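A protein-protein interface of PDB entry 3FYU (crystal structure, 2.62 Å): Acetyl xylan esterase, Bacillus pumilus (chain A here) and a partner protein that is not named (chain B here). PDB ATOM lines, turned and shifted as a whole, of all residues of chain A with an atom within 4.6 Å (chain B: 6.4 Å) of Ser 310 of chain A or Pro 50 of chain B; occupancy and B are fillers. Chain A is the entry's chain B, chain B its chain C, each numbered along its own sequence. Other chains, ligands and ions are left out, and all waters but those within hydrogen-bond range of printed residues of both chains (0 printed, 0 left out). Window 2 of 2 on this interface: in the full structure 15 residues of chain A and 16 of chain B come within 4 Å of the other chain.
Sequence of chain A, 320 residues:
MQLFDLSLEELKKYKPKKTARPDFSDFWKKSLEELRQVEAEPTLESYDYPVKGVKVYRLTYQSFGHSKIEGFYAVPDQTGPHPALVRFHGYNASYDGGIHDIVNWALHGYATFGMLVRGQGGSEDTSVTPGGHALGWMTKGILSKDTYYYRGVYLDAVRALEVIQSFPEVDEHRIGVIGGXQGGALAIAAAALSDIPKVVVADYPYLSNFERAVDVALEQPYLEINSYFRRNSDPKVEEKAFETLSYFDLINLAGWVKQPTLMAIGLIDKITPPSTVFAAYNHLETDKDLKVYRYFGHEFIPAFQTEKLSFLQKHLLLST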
ATOM      1  N   HIS A 108      10.349  31.876  10.735  1.00  0.00           N
ATOM      2  CA  HIS A 108       9.101  31.861   9.987  1.00  0.00           C
ATOM      3  C   HIS A 108       8.249  33.043  10.420  1.00  0.00           C
ATOM      4  O   HIS A 108       7.158  33.251   9.890  1.00  0.00           O
ATOM      5  CB  HIS A 108       8.353  30.552  10.217  1.00  0.00           C
ATOM      6  CG  HIS A 108       8.846  29.429   9.359  1.00  0.00           C
ATOM      7  ND1 HIS A 108       8.242  29.082   8.170  1.00  0.00           N
ATOM      8  CD2 HIS A 108       9.909  28.600   9.499  1.00  0.00           C
ATOM      9  CE1 HIS A 108       8.912  28.087   7.615  1.00  0.00           C
ATOM     10  NE2 HIS A 108       9.928  27.777   8.401  1.00  0.00           N
ATOM     11  N   THR A 306       3.467  21.371   5.549  1.00  0.00           N
ATOM     12  CA  THR A 306       2.924  22.396   4.668  1.00  0.00           C
ATOM     13  C   THR A 306       1.588  22.842   5.247  1.00  0.00           C
ATOM     14  O   THR A 306       1.349  24.037   5.421  1.00  0.00           O
ATOM     15  CB  THR A 306       2.692  21.862   3.226  1.00  0.00           C
ATOM     16  OG1 THR A 306       3.928  21.392   2.676  1.00  0.00           O
ATOM     17  CG2 THR A 306       2.159  22.961   2.341  1.00  0.00           C
ATOM     18  N   GLU A 307       0.724  21.869   5.544  1.00  0.00           N
ATOM     19  CA  GLU A 307      -0.595  22.128   6.132  1.00  0.00           C
ATOM     20  C   GLU A 307      -0.452  23.015   7.373  1.00  0.00           C
ATOM     21  O   GLU A 307      -1.143  24.031   7.515  1.00  0.00           O
ATOM     22  CB  GLU A 307      -1.260  20.813   6.546  1.00  0.00           C
ATOM     23  CG  GLU A 307      -1.648  19.908   5.401  1.00  0.00           C
ATOM     24  CD  GLU A 307      -2.808  20.460   4.594  1.00  0.00           C
ATOM     25  OE1 GLU A 307      -3.386  21.491   5.006  1.00  0.00           O
ATOM     26  OE2 GLU A 307      -3.146  19.857   3.550  1.00  0.00           O
ATOM     27  N   LYS A 308       0.451  22.604   8.259  1.00  0.00           N
ATOM     28  CA  LYS A 308       0.739  23.309   9.491  1.00  0.00           C
ATOM     29  C   LYS A 308       1.192  24.755   9.234  1.00  0.00           C
ATOM     30  O   LYS A 308       0.614  25.712   9.772  1.00  0.00           O
ATOM     31  CB  LYS A 308       1.815  22.545  10.256  1.00  0.00           C
ATOM     32  CG  LYS A 308       2.166  23.122  11.597  1.00  0.00           C
ATOM     33  CD  LYS A 308       3.281  22.319  12.271  1.00  0.00           C
ATOM     34  CE  LYS A 308       2.869  20.879  12.532  1.00  0.00           C
ATOM     35  NZ  LYS A 308       3.909  20.165  13.303  1.00  0.00           N
ATOM     36  N   LEU A 309       2.224  24.919   8.413  1.00  0.00           N
ATOM     37  CA  LEU A 309       2.737  26.252   8.109  1.00  0.00           C
ATOM     38  C   LEU A 309       1.660  27.119   7.481  1.00  0.00           C
ATOM     39  O   LEU A 309       1.551  28.314   7.767  1.00  0.00           O
ATOM     40  CB  LEU A 309       3.925  26.157   7.158  1.00  0.00           C
ATOM     41  CG  LEU A 309       5.175  25.510   7.749  1.00  0.00           C
ATOM     42  CD1 LEU A 309       6.237  25.329   6.670  1.00  0.00           C
ATOM     43  CD2 LEU A 309       5.687  26.383   8.881  1.00  0.00           C
ATOM     44  N   SER A 310       0.862  26.507   6.620  1.00  0.00           N
ATOM     45  CA  SER A 310      -0.198  27.232   5.940  1.00  0.00           C
ATOM     46  C   SER A 310      -1.307  27.652   6.904  1.00  0.00           C
ATOM     47  O   SER A 310      -1.846  28.760   6.808  1.00  0.00           O
ATOM     48  CB  SER A 310      -0.771  26.373   4.821  1.00  0.00           C
ATOM     49  OG  SER A 310      -1.823  27.065   4.187  1.00  0.00           O
ATOM     50  N   PHE A 311      -1.644  26.752   7.822  1.00  0.00           N
ATOM     51  CA  PHE A 311      -2.673  27.000   8.818  1.00  0.00           C
ATOM     52  C   PHE A 311      -2.237  28.128   9.756  1.00  0.00           C
ATOM     53  O   PHE A 311      -2.966  29.099   9.956  1.00  0.00           O
ATOM     54  CB  PHE A 311      -2.931  25.702   9.589  1.00  0.00           C
ATOM     55  CG  PHE A 311      -3.868  25.847  10.754  1.00  0.00           C
ATOM     56  CD1 PHE A 311      -3.373  26.084  12.040  1.00  0.00           C
ATOM     57  CD2 PHE A 311      -5.245  25.694  10.580  1.00  0.00           C
ATOM     58  CE1 PHE A 311      -4.238  26.158  13.134  1.00  0.00           C
ATOM     59  CE2 PHE A 311      -6.116  25.766  11.668  1.00  0.00           C
ATOM     60  CZ  PHE A 311      -5.612  25.995  12.944  1.00  0.00           C
ATOM     61  N   LEU A 312      -1.035  28.009  10.306  1.00  0.00           N
ATOM     62  CA  LEU A 312      -0.518  29.029  11.215  1.00  0.00           C
ATOM     63  C   LEU A 312      -0.375  30.378  10.533  1.00  0.00           C
ATOM     64  O   LEU A 312      -0.634  31.426  11.137  1.00  0.00           O
ATOM     65  CB  LEU A 312       0.835  28.606  11.775  1.00  0.00           C
ATOM     66  CG  LEU A 312       0.777  27.430  12.745  1.00  0.00           C
ATOM     67  CD1 LEU A 312       2.199  27.037  13.153  1.00  0.00           C
ATOM     68  CD2 LEU A 312      -0.073  27.807  13.957  1.00  0.00           C
ATOM     69  N   GLN A 313       0.035  30.344   9.273  1.00  0.00           N
ATOM     70  CA  GLN A 313       0.228  31.562   8.508  1.00  0.00           C
ATOM     71  C   GLN A 313      -1.098  32.276   8.352  1.00  0.00           C
ATOM     72  O   GLN A 313      -1.209  33.488   8.554  1.00  0.00           O
ATOM     73  CB  GLN A 313       0.798  31.226   7.138  1.00  0.00           C
ATOM     74  CG  GLN A 313       1.316  32.418   6.389  1.00  0.00           C
ATOM     75  CD  GLN A 313       2.088  32.019   5.155  1.00  0.00           C
ATOM     76  OE1 GLN A 313       1.525  31.448   4.223  1.00  0.00           O
ATOM     77  NE2 GLN A 313       3.387  32.311   5.145  1.00  0.00           N
ATOM     78  N   LYS A 314      -2.115  31.500   8.011  1.00  0.00           N
ATOM     79  CA  LYS A 314      -3.455  32.027   7.804  1.00  0.00           C
ATOM     80  C   LYS A 314      -4.082  32.635   9.054  1.00  0.00           C
ATOM     81  O   LYS A 314      -4.714  33.681   8.981  1.00  0.00           O
ATOM     82  CB  LYS A 314      -4.348  30.913   7.266  1.00  0.00           C
ATOM     83  CG  LYS A 314      -5.824  31.176   7.398  1.00  0.00           C
ATOM     84  CD  LYS A 314      -6.607  29.945   6.997  1.00  0.00           C
ATOM     85  CE  LYS A 314      -8.100  30.127   7.242  1.00  0.00           C
ATOM     86  NZ  LYS A 314      -8.892  28.989   6.681  1.00  0.00           N
ATOM     87  N   ASP B  48       4.681  27.897  -4.917  1.00  0.00           N
ATOM     88  CA  ASP B  48       4.046  28.401  -3.708  1.00  0.00           C
ATOM     89  C   ASP B  48       4.413  27.580  -2.496  1.00  0.00           C
ATOM     90  O   ASP B  48       4.449  26.357  -2.558  1.00  0.00           O
ATOM     91  CB  ASP B  48       2.521  28.420  -3.842  1.00  0.00           C
ATOM     92  CG  ASP B  48       2.035  29.472  -4.817  1.00  0.00           C
ATOM     93  OD1 ASP B  48       2.661  30.554  -4.876  1.00  0.00           O
ATOM     94  OD2 ASP B  48       1.020  29.224  -5.513  1.00  0.00           O
ATOM     95  N   TYR B  49       4.685  28.274  -1.399  1.00  0.00           N
ATOM     96  CA  TYR B  49       5.029  27.646  -0.136  1.00  0.00           C
ATOM     97  C   TYR B  49       4.620  28.602   0.987  1.00  0.00           C
ATOM     98  O   TYR B  49       4.896  29.799   0.918  1.00  0.00           O
ATOM     99  CB  TYR B  49       6.528  27.364  -0.080  1.00  0.00           C
ATOM    100  CG  TYR B  49       6.950  26.590   1.139  1.00  0.00           C
ATOM    101  CD1 TYR B  49       7.203  27.237   2.352  1.00  0.00           C
ATOM    102  CD2 TYR B  49       7.104  25.201   1.083  1.00  0.00           C
ATOM    103  CE1 TYR B  49       7.604  26.515   3.477  1.00  0.00           C
ATOM    104  CE2 TYR B  49       7.502  24.474   2.194  1.00  0.00           C
ATOM    105  CZ  TYR B  49       7.754  25.134   3.385  1.00  0.00           C
ATOM    106  OH  TYR B  49       8.179  24.407   4.472  1.00  0.00           O
ATOM    107  N   PRO B  50       3.951  28.088   2.031  1.00  0.00           N
ATOM    108  CA  PRO B  50       3.506  28.913   3.160  1.00  0.00           C
ATOM    109  C   PRO B  50       4.639  29.466   4.018  1.00  0.00           C
ATOM    110  O   PRO B  50       4.840  29.030   5.149  1.00  0.00           O
ATOM    111  CB  PRO B  50       2.615  27.965   3.944  1.00  0.00           C
ATOM    112  CG  PRO B  50       3.322  26.670   3.776  1.00  0.00           C
ATOM    113  CD  PRO B  50       3.651  26.669   2.279  1.00  0.00           C
ATOM    114  N   VAL B  51       5.379  30.424   3.475  1.00  0.00           N
ATOM    115  CA  VAL B  51       6.480  31.044   4.195  1.00  0.00           C
ATOM    116  C   VAL B  51       6.560  32.523   3.829  1.00  0.00           C
ATOM    117  O   VAL B  51       6.173  32.932   2.734  1.00  0.00           O
ATOM    118  CB  VAL B  51       7.833  30.367   3.870  1.00  0.00           C
ATOM    119  CG1 VAL B  51       8.201  30.624   2.425  1.00  0.00           C
ATOM    120  CG2 VAL B  51       8.923  30.890   4.798  1.00  0.00           C
ATOM    121  N   LYS B  52       7.062  33.325   4.753  1.00  0.00           N
ATOM    122  CA  LYS B  52       7.183  34.757   4.542  1.00  0.00           C
ATOM    123  C   LYS B  52       8.655  35.080   4.502  1.00  0.00           C
ATOM    124  O   LYS B  52       9.429  34.525   5.283  1.00  0.00           O
ATOM    125  CB  LYS B  52       6.502  35.487   5.695  1.00  0.00           C
ATOM    126  CG  LYS B  52       6.595  36.996   5.697  1.00  0.00           C
ATOM    127  CD  LYS B  52       5.614  37.567   6.730  1.00  0.00           C
ATOM    128  CE  LYS B  52       5.683  39.087   6.852  1.00  0.00           C
ATOM    129  NZ  LYS B  52       6.902  39.536   7.587  1.00  0.00           N
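Among the printed residues, merely in contact across the chains: His 108 of chain A with Val 51 of chain B (3.9 Å), Thr 306 of chain A with Pro 50 of chain B (3.7 Å), Leu 309 of chain A with Tyr 49 of chain B (3.1 Å), Leu 309 of chain A with Pro 50 of chain B (3.5 Å), Ser 310 of chain A with Pro 50 of chain B (3.5 Å), Gln 313 of chain A with Pro 50 of chain B (3.3 Å) and Gln 313 of chain A with Lys 52 of chain B (3.8 Å).
The backbone NH (N) of Val 51 of chain B lies close to the side-chain amide nitrogen (NE2) of Gln 313 of chain A, at 3.2 Å.
Of the printed residues of chain B, His 108 of chain A touches Val 51 (3.9 Å).
Lys 308 of chain A touches none of the printed residues of chain B.
Of the printed residues of chain B, Ser 310 of chain A touches Pro 50.
Printed residues of chain B within 4 Å of Gln 313 of chain A: Pro 50 (3.3 Å), Val 51 (3.2 Å) and Lys 52 (3.8 Å).
Asp 48 of chain B touches none of the printed residues of chain A.
Of chain A, only Thr 306, Leu 309, Ser 310 and Gln 313 come within 4 Å of Pro 50 of chain B.
Of the printed residues of chain A, Val 51 of chain B touches His 108 (3.9 Å) and Gln 313 (3.2 Å).
Printed residues of chain A within 4 Å of Lys 52 of chain B: Gln 313 (3.8 Å).
The nearest printed residue of chain B that does not touch Ser 310 of chain A is Val 51 of chain B (6.8 Å).
The nearest printed residue of chain A that does not touch Pro 50 of chain B is His 108 of chain A (4.6 Å).
The nearest printed residue of chain A that does not touch Lys 52 of chain B is His 108 of chain A (4.8 Å).
Of the 5 printed residues of chain B, 4 touch a printed residue of chain A.
Printed residues of chain B that touch a printed residue of chain A: Tyr 49, Pro 50, Val 51 and Lys 52.
Hydrophobic or aromatic side chains of chain A within 4 Å of the printed part of chain B: His 108 and Leu 309.
Among the printed residues, 8 pairs touch across the chains.
Among the printed residues, no Asp or Glu carboxylate lies within 4 Å of a Lys or Arg side-chain nitrogen of the other chain.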
